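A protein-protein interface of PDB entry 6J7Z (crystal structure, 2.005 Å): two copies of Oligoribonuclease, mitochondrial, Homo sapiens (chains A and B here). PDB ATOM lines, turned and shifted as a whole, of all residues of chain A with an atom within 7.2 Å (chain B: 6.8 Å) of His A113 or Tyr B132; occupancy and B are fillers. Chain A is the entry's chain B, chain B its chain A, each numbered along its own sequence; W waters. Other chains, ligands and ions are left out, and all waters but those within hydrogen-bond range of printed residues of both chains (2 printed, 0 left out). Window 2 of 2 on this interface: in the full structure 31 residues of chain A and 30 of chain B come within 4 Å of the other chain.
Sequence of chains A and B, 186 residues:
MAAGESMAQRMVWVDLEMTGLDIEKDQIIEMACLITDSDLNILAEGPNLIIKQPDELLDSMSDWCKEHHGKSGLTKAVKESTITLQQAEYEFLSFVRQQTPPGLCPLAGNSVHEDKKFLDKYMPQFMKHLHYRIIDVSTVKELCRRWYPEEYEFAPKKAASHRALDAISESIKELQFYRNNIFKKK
The backbone carbonyl oxygen (O) of Ile B134 sits at hydrogen-bond distance from the side-chain hydroxyl (OG1) of Thr A139, 2.9 Å away.
NZ of Lys B117 lies within salt-bridge range of OD2 of Asp A120, at 3.4 Å.
N of Asp B136 lies within hydrogen-bond range of OG1 of Thr A139 (2.9 Å).
The side-chain carboxylate (OE1) of Glu B114 is in salt-bridge range of the side-chain amino group (NZ) of Lys A116 (3.6 Å).
ND1 of His B131 sits at hydrogen-bond distance from N of Arg B133, at 3.0 Å.
The backbone NH (N) of Ser A111 lies within hydrogen-bond range of the side-chain carboxylate (OD1) of Asp A136 (2.8 Å).
The side-chain amino group (NZ) of Lys A116 lies within salt-bridge range of the side-chain carboxylate (OD2) of Asp A120, at 2.9 Å.
The backbone NH (N) of Ser A138 is in hydrogen-bond range of the side-chain carboxylate (OD1) of Asp A136 (2.9 Å).
OG of Ser A138 lies within hydrogen-bond range of OG of Ser A111, 3.1 Å away.
Ser A111 touches Tyr B132.
CG of Arg B133 touches OG of Ser A111, at 3.6 Å.
His A113 touches His B113 (CB to CB, 3.8 Å).
His A113 touches Tyr B132.
CD2 of His A113 touches CD1 of Ile B134, 3.5 Å away.
Ile A134 touches His B113.
Asp B136 touches Ile A134 (OD2 to CG1, 3.7 Å).
Asp A136 touches Ile B134.
Lys A141 touches Arg B133 (CD to CZ, 3.5 Å).
His A113 touches three residues of chain B.
Tyr B132 touches two residues of chain A.
Of the printed residues of chain B, Asp A120 touches Lys B117.
Of the printed residues of chain A, Asp B136 touches Ile A134 and Thr A139.
Of the printed residues of chain A, Ile B134 touches His A113 (3.5 Å), Asp A136 (3.6 Å) and Thr A139 (2.9 Å).
Val A112 touches none of the printed residues of chain B.
Ser A138 touches none of the printed residues of chain B.
The nearest residue of chain B that does not touch His A113 is Lys B116 (4.3 Å).
The nearest residue of chain A that does not touch Tyr B132 is Ser A138 (6.0 Å).
Hydrophobic or aromatic side chains of chain B within 4 Å of the printed part of chain A: His B113, Tyr B132 and Ile B134.
Along chain B the printed residues that touch a printed residue of chain A span positions 113 to 136.
Of the 18 printed residues of chain A, 8 touch a printed residue of chain B.
Along chain A the printed residues that touch a printed residue of chain B span positions 111 to 141.
Among the printed residues, Asp or Glu carboxylates within 4 Å of a Lys or Arg side-chain nitrogen of the other chain: Lys A116 with Glu B114 (3.6 Å) and Asp A120 with Lys B117 (3.4 Å).
His A113 touches Ile B134, and with the chains exchanged Ile A134 touches His B113.
Lys A116 touches Glu B114, but with the chains exchanged Glu A114 does not touch Lys B116 (4.8 Å).
Asp A120 touches Lys B117, but with the chains exchanged Lys A117 does not touch Asp B120 (4.4 Å).
Ile A134 touches Asp B136, and with the chains exchanged Asp A136 touches Ile B134.
Of the 13 pairs that touch across the chains among the printed residues, 5 have their exchanged pair printed and touching as well.
Water W2 lies within hydrogen-bond range of the side-chain carboxylate of Asp A136 (2.5 Å), the backbone NH of Ile B134 (3.0 Å), a ring nitrogen (NE2) of His A113 (3.1 Å) and the side-chain hydroxyl of Ser A111 (3.1 Å).
Water W1 bridges the backbone carbonyl oxygen of Lys A117 (2.9 Å) and the side-chain amino group of Lys B117 (3.5 Å).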
ATOM      1  N   LEU A 107     -16.419 -34.957  24.356  1.00  0.00           N
ATOM      2  CA  LEU A 107     -15.786 -33.664  24.574  1.00  0.00           C
ATOM      3  C   LEU A 107     -16.536 -32.583  23.809  1.00  0.00           C
ATOM      4  O   LEU A 107     -17.034 -32.814  22.703  1.00  0.00           O
ATOM      5  CB  LEU A 107     -14.327 -33.702  24.114  1.00  0.00           C
ATOM      6  CG  LEU A 107     -13.207 -33.763  25.152  1.00  0.00           C
ATOM      7  CD1 LEU A 107     -11.877 -33.410  24.502  1.00  0.00           C
ATOM      8  CD2 LEU A 107     -13.500 -32.840  26.316  1.00  0.00           C
ATOM      9  N   GLY A 109     -16.697 -28.077  23.060  1.00  0.00           N
ATOM     10  CA  GLY A 109     -16.021 -26.798  23.111  1.00  0.00           C
ATOM     11  C   GLY A 109     -15.864 -26.220  21.721  1.00  0.00           C
ATOM     12  O   GLY A 109     -16.315 -26.792  20.727  1.00  0.00           O
ATOM     13  N   ASN A 110     -15.213 -25.060  21.674  1.00  0.00           N
ATOM     14  CA  ASN A 110     -14.920 -24.379  20.418  1.00  0.00           C
ATOM     15  C   ASN A 110     -13.618 -24.923  19.844  1.00  0.00           C
ATOM     16  O   ASN A 110     -12.570 -24.830  20.491  1.00  0.00           O
ATOM     17  CB  ASN A 110     -14.815 -22.869  20.629  1.00  0.00           C
ATOM     18  CG  ASN A 110     -16.143 -22.161  20.464  1.00  0.00           C
ATOM     19  OD1 ASN A 110     -16.719 -21.668  21.431  1.00  0.00           O
ATOM     20  ND2 ASN A 110     -16.635 -22.106  19.231  1.00  0.00           N
ATOM     21  N   SER A 111     -13.686 -25.474  18.631  1.00  0.00           N
ATOM     22  CA  SER A 111     -12.530 -26.089  17.974  1.00  0.00           C
ATOM     23  C   SER A 111     -11.830 -27.065  18.918  1.00  0.00           C
ATOM     24  O   SER A 111     -10.606 -27.059  19.072  1.00  0.00           O
ATOM     25  CB  SER A 111     -11.558 -25.023  17.464  1.00  0.00           C
ATOM     26  OG  SER A 111     -12.119 -24.288  16.391  1.00  0.00           O
ATOM     27  N   VAL A 112     -12.633 -27.922  19.549  1.00  0.00           N
ATOM     28  CA  VAL A 112     -12.181 -28.743  20.669  1.00  0.00           C
ATOM     29  C   VAL A 112     -11.278 -29.881  20.204  1.00  0.00           C
ATOM     30  O   VAL A 112     -10.763 -30.643  21.027  1.00  0.00           O
ATOM     31  CB  VAL A 112     -13.397 -29.278  21.454  1.00  0.00           C
ATOM     32  CG1 VAL A 112     -13.989 -30.500  20.763  1.00  0.00           C
ATOM     33  CG2 VAL A 112     -13.024 -29.572  22.906  1.00  0.00           C
ATOM     34  N   HIS A 113     -11.065 -30.003  18.891  1.00  0.00           N
ATOM     35  CA  HIS A 113     -10.151 -31.032  18.400  1.00  0.00           C
ATOM     36  C   HIS A 113      -8.707 -30.745  18.803  1.00  0.00           C
ATOM     37  O   HIS A 113      -7.934 -31.678  19.050  1.00  0.00           O
ATOM     38  CB  HIS A 113     -10.264 -31.170  16.879  1.00  0.00           C
ATOM     39  CG  HIS A 113     -10.423 -29.867  16.163  1.00  0.00           C
ATOM     40  ND1 HIS A 113      -9.350 -29.136  15.700  1.00  0.00           N
ATOM     41  CD2 HIS A 113     -11.529 -29.163  15.827  1.00  0.00           C
ATOM     42  CE1 HIS A 113      -9.787 -28.036  15.112  1.00  0.00           C
ATOM     43  NE2 HIS A 113     -11.107 -28.029  15.176  1.00  0.00           N
ATOM     44  N   GLU A 114      -8.327 -29.469  18.892  1.00  0.00           N
ATOM     45  CA  GLU A 114      -6.993 -29.121  19.375  1.00  0.00           C
ATOM     46  C   GLU A 114      -6.831 -29.484  20.847  1.00  0.00           C
ATOM     47  O   GLU A 114      -5.805 -30.054  21.257  1.00  0.00           O
ATOM     48  CB  GLU A 114      -6.737 -27.628  19.154  1.00  0.00           C
ATOM     49  CG  GLU A 114      -5.317 -27.180  19.449  1.00  0.00           C
ATOM     50  CD  GLU A 114      -4.353 -27.532  18.335  1.00  0.00           C
ATOM     51  OE1 GLU A 114      -4.821 -27.907  17.239  1.00  0.00           O
ATOM     52  OE2 GLU A 114      -3.127 -27.436  18.554  1.00  0.00           O
ATOM     53  N   ASP A 115      -7.832 -29.140  21.662  1.00  0.00           N
ATOM     54  CA  ASP A 115      -7.831 -29.560  23.059  1.00  0.00           C
ATOM     55  C   ASP A 115      -7.755 -31.075  23.166  1.00  0.00           C
ATOM     56  O   ASP A 115      -7.067 -31.607  24.042  1.00  0.00           O
ATOM     57  CB  ASP A 115      -9.080 -29.039  23.771  1.00  0.00           C
ATOM     58  CG  ASP A 115      -9.270 -27.546  23.600  1.00  0.00           C
ATOM     59  OD1 ASP A 115      -9.735 -27.126  22.519  1.00  0.00           O
ATOM     60  OD2 ASP A 115      -8.958 -26.794  24.547  1.00  0.00           O
ATOM     61  N   LYS A 116      -8.450 -31.787  22.276  1.00  0.00           N
ATOM     62  CA  LYS A 116      -8.414 -33.244  22.300  1.00  0.00           C
ATOM     63  C   LYS A 116      -7.028 -33.767  21.949  1.00  0.00           C
ATOM     64  O   LYS A 116      -6.573 -34.758  22.525  1.00  0.00           O
ATOM     65  CB  LYS A 116      -9.458 -33.819  21.345  1.00  0.00           C
ATOM     66  CG  LYS A 116      -9.426 -35.336  21.252  1.00  0.00           C
ATOM     67  CD  LYS A 116     -10.602 -35.878  20.459  1.00  0.00           C
ATOM     68  CE  LYS A 116     -10.564 -37.396  20.396  1.00  0.00           C
ATOM     69  NZ  LYS A 116      -9.313 -37.895  19.762  1.00  0.00           N
ATOM     70  N   LYS A 117      -6.347 -33.123  21.002  1.00  0.00           N
ATOM     71  CA  LYS A 117      -4.971 -33.501  20.689  1.00  0.00           C
ATOM     72  C   LYS A 117      -4.078 -33.363  21.919  1.00  0.00           C
ATOM     73  O   LYS A 117      -3.363 -34.304  22.303  1.00  0.00           O
ATOM     74  CB  LYS A 117      -4.449 -32.640  19.537  1.00  0.00           C
ATOM     75  CG  LYS A 117      -3.019 -32.933  19.111  1.00  0.00           C
ATOM     76  CD  LYS A 117      -2.665 -32.203  17.820  1.00  0.00           C
ATOM     77  CE  LYS A 117      -2.733 -30.692  17.994  1.00  0.00           C
ATOM     78  NZ  LYS A 117      -2.523 -29.968  16.709  1.00  0.00           N
ATOM     79  N   PHE A 118      -4.126 -32.194  22.561  1.00  0.00           N
ATOM     80  CA  PHE A 118      -3.272 -31.971  23.726  1.00  0.00           C
ATOM     81  C   PHE A 118      -3.632 -32.898  24.884  1.00  0.00           C
ATOM     82  O   PHE A 118      -2.741 -33.351  25.612  1.00  0.00           O
ATOM     83  CB  PHE A 118      -3.342 -30.509  24.161  1.00  0.00           C
ATOM     84  CG  PHE A 118      -2.369 -29.621  23.440  1.00  0.00           C
ATOM     85  CD1 PHE A 118      -2.708 -29.041  22.228  1.00  0.00           C
ATOM     86  CD2 PHE A 118      -1.110 -29.380  23.964  1.00  0.00           C
ATOM     87  CE1 PHE A 118      -1.811 -28.230  21.557  1.00  0.00           C
ATOM     88  CE2 PHE A 118      -0.210 -28.570  23.299  1.00  0.00           C
ATOM     89  CZ  PHE A 118      -0.560 -27.993  22.094  1.00  0.00           C
ATOM     90  N   LEU A 119      -4.919 -33.212  25.055  1.00  0.00           N
ATOM     91  CA  LEU A 119      -5.329 -34.098  26.141  1.00  0.00           C
ATOM     92  C   LEU A 119      -4.955 -35.546  25.846  1.00  0.00           C
ATOM     93  O   LEU A 119      -4.543 -36.281  26.750  1.00  0.00           O
ATOM     94  CB  LEU A 119      -6.833 -33.968  26.382  1.00  0.00           C
ATOM     95  CG  LEU A 119      -7.323 -32.659  27.007  1.00  0.00           C
ATOM     96  CD1 LEU A 119      -8.845 -32.592  26.995  1.00  0.00           C
ATOM     97  CD2 LEU A 119      -6.783 -32.502  28.418  1.00  0.00           C
ATOM     98  N   ASP A 120      -5.104 -35.978  24.591  1.00  0.00           N
ATOM     99  CA  ASP A 120      -4.657 -37.308  24.201  1.00  0.00           C
ATOM    100  C   ASP A 120      -3.168 -37.473  24.455  1.00  0.00           C
ATOM    101  O   ASP A 120      -2.715 -38.552  24.857  1.00  0.00           O
ATOM    102  CB  ASP A 120      -4.968 -37.558  22.724  1.00  0.00           C
ATOM    103  CG  ASP A 120      -6.429 -37.877  22.476  1.00  0.00           C
ATOM    104  OD1 ASP A 120      -7.092 -38.407  23.392  1.00  0.00           O
ATOM    105  OD2 ASP A 120      -6.913 -37.600  21.359  1.00  0.00           O
ATOM    106  N   ILE A 134     -16.758 -35.861  19.158  1.00  0.00           N
ATOM    107  CA  ILE A 134     -16.682 -34.536  19.754  1.00  0.00           C
ATOM    108  C   ILE A 134     -17.898 -33.728  19.322  1.00  0.00           C
ATOM    109  O   ILE A 134     -18.561 -34.028  18.326  1.00  0.00           O
ATOM    110  CB  ILE A 134     -15.383 -33.794  19.376  1.00  0.00           C
ATOM    111  CG1 ILE A 134     -15.342 -33.531  17.867  1.00  0.00           C
ATOM    112  CG2 ILE A 134     -14.163 -34.585  19.827  1.00  0.00           C
ATOM    113  CD1 ILE A 134     -14.297 -32.519  17.441  1.00  0.00           C
ATOM    114  N   ASP A 136     -18.205 -30.035  18.335  1.00  0.00           N
ATOM    115  CA  ASP A 136     -17.424 -28.846  18.016  1.00  0.00           C
ATOM    116  C   ASP A 136     -18.379 -27.693  17.737  1.00  0.00           C
ATOM    117  O   ASP A 136     -19.075 -27.685  16.716  1.00  0.00           O
ATOM    118  CB  ASP A 136     -16.509 -29.111  16.824  1.00  0.00           C
ATOM    119  CG  ASP A 136     -15.554 -27.964  16.545  1.00  0.00           C
ATOM    120  OD1 ASP A 136     -15.607 -26.941  17.263  1.00  0.00           O
ATOM    121  OD2 ASP A 136     -14.747 -28.086  15.600  1.00  0.00           O
ATOM    122  N   SER A 138     -17.529 -24.806  16.881  1.00  0.00           N
ATOM    123  CA  SER A 138     -17.043 -24.030  15.745  1.00  0.00           C
ATOM    124  C   SER A 138     -17.587 -24.553  14.421  1.00  0.00           C
ATOM    125  O   SER A 138     -17.721 -23.783  13.463  1.00  0.00           O
ATOM    126  CB  SER A 138     -15.515 -24.021  15.733  1.00  0.00           C
ATOM    127  OG  SER A 138     -15.010 -23.233  16.798  1.00  0.00           O
ATOM    128  N   THR A 139     -17.912 -25.846  14.345  1.00  0.00           N
ATOM    129  CA  THR A 139     -18.602 -26.364  13.167  1.00  0.00           C
ATOM    130  C   THR A 139     -19.946 -25.670  12.980  1.00  0.00           C
ATOM    131  O   THR A 139     -20.276 -25.198  11.882  1.00  0.00           O
ATOM    132  CB  THR A 139     -18.791 -27.877  13.295  1.00  0.00           C
ATOM    133  OG1 THR A 139     -17.527 -28.538  13.147  1.00  0.00           O
ATOM    134  CG2 THR A 139     -19.753 -28.390  12.233  1.00  0.00           C
ATOM    135  N   LYS A 141     -20.675 -22.840  14.208  1.00  0.00           N
ATOM    136  CA  LYS A 141     -20.381 -21.433  13.957  1.00  0.00           C
ATOM    137  C   LYS A 141     -20.150 -21.176  12.473  1.00  0.00           C
ATOM    138  O   LYS A 141     -20.678 -20.214  11.905  1.00  0.00           O
ATOM    139  CB  LYS A 141     -19.163 -21.003  14.775  1.00  0.00           C
ATOM    140  CG  LYS A 141     -18.597 -19.646  14.393  1.00  0.00           C
ATOM    141  CD  LYS A 141     -17.091 -19.602  14.602  1.00  0.00           C
ATOM    142  CE  LYS A 141     -16.723 -19.859  16.056  1.00  0.00           C
ATOM    143  NZ  LYS A 141     -17.159 -18.747  16.946  1.00  0.00           N
ATOM    144  N   GLY B 103      -5.767 -20.052   3.684  1.00  0.00           N
ATOM    145  CA  GLY B 103      -6.099 -19.947   5.089  1.00  0.00           C
ATOM    146  C   GLY B 103      -7.550 -19.670   5.417  1.00  0.00           C
ATOM    147  O   GLY B 103      -7.876 -19.524   6.602  1.00  0.00           O
ATOM    148  N   CYS B 105     -10.540 -21.450   4.099  1.00  0.00           N
ATOM    149  CA  CYS B 105     -11.578 -22.463   3.993  1.00  0.00           C
ATOM    150  C   CYS B 105     -11.279 -23.666   4.885  1.00  0.00           C
ATOM    151  O   CYS B 105     -10.117 -24.041   5.074  1.00  0.00           O
ATOM    152  CB  CYS B 105     -11.738 -22.931   2.542  1.00  0.00           C
ATOM    153  SG  CYS B 105     -12.310 -21.622   1.429  1.00  0.00           S
ATOM    154  N   PRO B 106     -12.310 -24.289   5.448  1.00  0.00           N
ATOM    155  CA  PRO B 106     -12.100 -25.386   6.393  1.00  0.00           C
ATOM    156  C   PRO B 106     -12.179 -26.769   5.764  1.00  0.00           C
ATOM    157  O   PRO B 106     -12.815 -26.995   4.727  1.00  0.00           O
ATOM    158  CB  PRO B 106     -13.256 -25.189   7.382  1.00  0.00           C
ATOM    159  CG  PRO B 106     -14.363 -24.674   6.525  1.00  0.00           C
ATOM    160  CD  PRO B 106     -13.717 -23.853   5.424  1.00  0.00           C
ATOM    161  N   LEU B 107     -11.507 -27.701   6.441  1.00  0.00           N
ATOM    162  CA  LEU B 107     -11.677 -29.121   6.179  1.00  0.00           C
ATOM    163  C   LEU B 107     -13.094 -29.557   6.533  1.00  0.00           C
ATOM    164  O   LEU B 107     -13.718 -29.036   7.461  1.00  0.00           O
ATOM    165  CB  LEU B 107     -10.672 -29.938   6.993  1.00  0.00           C
ATOM    166  CG  LEU B 107      -9.417 -30.469   6.303  1.00  0.00           C
ATOM    167  CD1 LEU B 107      -8.903 -31.702   7.030  1.00  0.00           C
ATOM    168  CD2 LEU B 107      -9.711 -30.778   4.854  1.00  0.00           C
ATOM    169  N   HIS B 113     -11.950 -34.638  12.380  1.00  0.00           N
ATOM    170  CA  HIS B 113     -10.879 -34.270  13.300  1.00  0.00           C
ATOM    171  C   HIS B 113      -9.760 -35.307  13.310  1.00  0.00           C
ATOM    172  O   HIS B 113      -8.588 -34.944  13.446  1.00  0.00           O
ATOM    173  CB  HIS B 113     -11.432 -34.058  14.710  1.00  0.00           C
ATOM    174  CG  HIS B 113     -12.406 -35.108  15.149  1.00  0.00           C
ATOM    175  ND1 HIS B 113     -13.726 -35.113  14.752  1.00  0.00           N
ATOM    176  CD2 HIS B 113     -12.253 -36.178  15.963  1.00  0.00           C
ATOM    177  CE1 HIS B 113     -14.343 -36.145  15.298  1.00  0.00           C
ATOM    178  NE2 HIS B 113     -13.472 -36.809  16.036  1.00  0.00           N
ATOM    179  N   GLU B 114     -10.087 -36.591  13.140  1.00  0.00           N
ATOM    180  CA  GLU B 114      -9.040 -37.608  13.051  1.00  0.00           C
ATOM    181  C   GLU B 114      -8.225 -37.450  11.771  1.00  0.00           C
ATOM    182  O   GLU B 114      -6.987 -37.543  11.792  1.00  0.00           O
ATOM    183  CB  GLU B 114      -9.660 -39.002  13.125  1.00  0.00           C
ATOM    184  CG  GLU B 114      -9.988 -39.466  14.536  1.00  0.00           C
ATOM    185  CD  GLU B 114      -8.761 -39.550  15.421  1.00  0.00           C
ATOM    186  OE1 GLU B 114      -8.615 -38.697  16.322  1.00  0.00           O
ATOM    187  OE2 GLU B 114      -7.940 -40.469  15.215  1.00  0.00           O
ATOM    188  N   LYS B 116      -7.803 -34.694  10.207  1.00  0.00           N
ATOM    189  CA  LYS B 116      -6.992 -33.499  10.405  1.00  0.00           C
ATOM    190  C   LYS B 116      -5.793 -33.789  11.299  1.00  0.00           C
ATOM    191  O   LYS B 116      -4.709 -33.240  11.084  1.00  0.00           O
ATOM    192  CB  LYS B 116      -7.835 -32.371  10.997  1.00  0.00           C
ATOM    193  CG  LYS B 116      -7.066 -31.069  11.167  1.00  0.00           C
ATOM    194  CD  LYS B 116      -7.942 -29.975  11.737  1.00  0.00           C
ATOM    195  CE  LYS B 116      -7.267 -28.617  11.644  1.00  0.00           C
ATOM    196  NZ  LYS B 116      -6.210 -28.454  12.678  1.00  0.00           N
ATOM    197  N   LYS B 117      -5.971 -34.643  12.308  1.00  0.00           N
ATOM    198  CA  LYS B 117      -4.844 -35.046  13.142  1.00  0.00           C
ATOM    199  C   LYS B 117      -3.774 -35.740  12.311  1.00  0.00           C
ATOM    200  O   LYS B 117      -2.575 -35.508  12.507  1.00  0.00           O
ATOM    201  CB  LYS B 117      -5.326 -35.958  14.271  1.00  0.00           C
ATOM    202  CG  LYS B 117      -4.213 -36.509  15.150  1.00  0.00           C
ATOM    203  CD  LYS B 117      -4.578 -36.415  16.622  1.00  0.00           C
ATOM    204  CE  LYS B 117      -4.219 -37.691  17.366  1.00  0.00           C
ATOM    205  NZ  LYS B 117      -4.744 -37.683  18.759  1.00  0.00           N
ATOM    206  N   ASP B 120      -2.250 -32.882   9.693  1.00  0.00           N
ATOM    207  CA  ASP B 120      -1.406 -31.873  10.326  1.00  0.00           C
ATOM    208  C   ASP B 120       0.014 -32.381  10.519  1.00  0.00           C
ATOM    209  O   ASP B 120       0.966 -31.595  10.486  1.00  0.00           O
ATOM    210  CB  ASP B 120      -1.998 -31.459  11.675  1.00  0.00           C
ATOM    211  CG  ASP B 120      -3.180 -30.522  11.535  1.00  0.00           C
ATOM    212  OD1 ASP B 120      -3.419 -30.018  10.418  1.00  0.00           O
ATOM    213  OD2 ASP B 120      -3.872 -30.289  12.549  1.00  0.00           O
ATOM    214  N   MET B 127      -2.210 -28.559   4.943  1.00  0.00           N
ATOM    215  CA  MET B 127      -3.071 -28.046   6.004  1.00  0.00           C
ATOM    216  C   MET B 127      -2.847 -26.559   6.252  1.00  0.00           C
ATOM    217  O   MET B 127      -3.776 -25.858   6.670  1.00  0.00           O
ATOM    218  CB  MET B 127      -2.847 -28.839   7.289  1.00  0.00           C
ATOM    219  CG  MET B 127      -3.240 -30.299   7.179  1.00  0.00           C
ATOM    220  SD  MET B 127      -4.934 -30.490   6.591  1.00  0.00           S
ATOM    221  CE  MET B 127      -5.840 -29.780   7.960  1.00  0.00           C
ATOM    222  N   LEU B 130      -5.276 -24.286   4.654  1.00  0.00           N
ATOM    223  CA  LEU B 130      -6.648 -24.352   5.130  1.00  0.00           C
ATOM    224  C   LEU B 130      -6.805 -23.592   6.442  1.00  0.00           C
ATOM    225  O   LEU B 130      -5.832 -23.294   7.139  1.00  0.00           O
ATOM    226  CB  LEU B 130      -7.077 -25.809   5.322  1.00  0.00           C
ATOM    227  CG  LEU B 130      -7.607 -26.624   4.139  1.00  0.00           C
ATOM    228  CD1 LEU B 130      -6.907 -26.288   2.832  1.00  0.00           C
ATOM    229  CD2 LEU B 130      -7.450 -28.098   4.448  1.00  0.00           C
ATOM    230  N   HIS B 131      -8.056 -23.280   6.770  1.00  0.00           N
ATOM    231  CA  HIS B 131      -8.375 -22.721   8.074  1.00  0.00           C
ATOM    232  C   HIS B 131      -8.118 -23.759   9.163  1.00  0.00           C
ATOM    233  O   HIS B 131      -8.003 -24.959   8.899  1.00  0.00           O
ATOM    234  CB  HIS B 131      -9.834 -22.262   8.111  1.00  0.00           C
ATOM    235  CG  HIS B 131     -10.112 -21.194   9.122  1.00  0.00           C
ATOM    236  ND1 HIS B 131     -10.521 -21.474  10.408  1.00  0.00           N
ATOM    237  CD2 HIS B 131     -10.049 -19.844   9.034  1.00  0.00           C
ATOM    238  CE1 HIS B 131     -10.693 -20.343  11.070  1.00  0.00           C
ATOM    239  NE2 HIS B 131     -10.413 -19.339  10.259  1.00  0.00           N
ATOM    240  N   TYR B 132      -8.017 -23.287  10.407  1.00  0.00           N
ATOM    241  CA  TYR B 132      -7.845 -24.217  11.515  1.00  0.00           C
ATOM    242  C   TYR B 132      -9.168 -24.802  11.990  1.00  0.00           C
ATOM    243  O   TYR B 132      -9.172 -25.875  12.602  1.00  0.00           O
ATOM    244  CB  TYR B 132      -7.109 -23.543  12.679  1.00  0.00           C
ATOM    245  CG  TYR B 132      -7.869 -22.440  13.383  1.00  0.00           C
ATOM    246  CD1 TYR B 132      -8.741 -22.724  14.428  1.00  0.00           C
ATOM    247  CD2 TYR B 132      -7.691 -21.110  13.022  1.00  0.00           C
ATOM    248  CE1 TYR B 132      -9.428 -21.717  15.080  1.00  0.00           C
ATOM    249  CE2 TYR B 132      -8.372 -20.097  13.669  1.00  0.00           C
ATOM    250  CZ  TYR B 132      -9.239 -20.406  14.697  1.00  0.00           C
ATOM    251  OH  TYR B 132      -9.919 -19.401  15.344  1.00  0.00           O
ATOM    252  N   ARG B 133     -10.283 -24.129  11.720  1.00  0.00           N
ATOM    253  CA  ARG B 133     -11.586 -24.681  12.047  1.00  0.00           C
ATOM    254  C   ARG B 133     -11.957 -25.785  11.063  1.00  0.00           C
ATOM    255  O   ARG B 133     -11.459 -25.848   9.936  1.00  0.00           O
ATOM    256  CB  ARG B 133     -12.656 -23.590  12.031  1.00  0.00           C
ATOM    257  CG  ARG B 133     -12.596 -22.645  13.214  1.00  0.00           C
ATOM    258  CD  ARG B 133     -13.478 -21.432  12.987  1.00  0.00           C
ATOM    259  NE  ARG B 133     -13.355 -20.462  14.069  1.00  0.00           N
ATOM    260  CZ  ARG B 133     -13.651 -19.173  13.950  1.00  0.00           C
ATOM    261  NH1 ARG B 133     -14.090 -18.697  12.792  1.00  0.00           N
ATOM    262  NH2 ARG B 133     -13.509 -18.360  14.988  1.00  0.00           N
ATOM    263  N   ILE B 134     -12.848 -26.669  11.510  1.00  0.00           N
ATOM    264  CA  ILE B 134     -13.324 -27.775  10.697  1.00  0.00           C
ATOM    265  C   ILE B 134     -14.843 -27.743  10.663  1.00  0.00           C
ATOM    266  O   ILE B 134     -15.500 -27.167  11.534  1.00  0.00           O
ATOM    267  CB  ILE B 134     -12.840 -29.146  11.218  1.00  0.00           C
ATOM    268  CG1 ILE B 134     -13.478 -29.457  12.575  1.00  0.00           C
ATOM    269  CG2 ILE B 134     -11.330 -29.176  11.316  1.00  0.00           C
ATOM    270  CD1 ILE B 134     -13.056 -30.787  13.160  1.00  0.00           C
ATOM    271  N   ASP B 136     -17.267 -30.487  11.051  1.00  0.00           N
ATOM    272  CA  ASP B 136     -17.394 -31.884  11.444  1.00  0.00           C
ATOM    273  C   ASP B 136     -18.860 -32.285  11.339  1.00  0.00           C
ATOM    274  O   ASP B 136     -19.688 -31.863  12.153  1.00  0.00           O
ATOM    275  CB  ASP B 136     -16.861 -32.086  12.860  1.00  0.00           C
ATOM    276  CG  ASP B 136     -17.014 -33.511  13.345  1.00  0.00           C
ATOM    277  OD1 ASP B 136     -17.045 -34.427  12.498  1.00  0.00           O
ATOM    278  OD2 ASP B 136     -17.099 -33.713  14.576  1.00  0.00           O
HETATM  279  O   HOH W   1      -2.107 -36.015  20.302  1.00  0.00           O
HETATM  280  O   HOH W   2     -13.506 -26.231  14.427  1.00  0.00           O
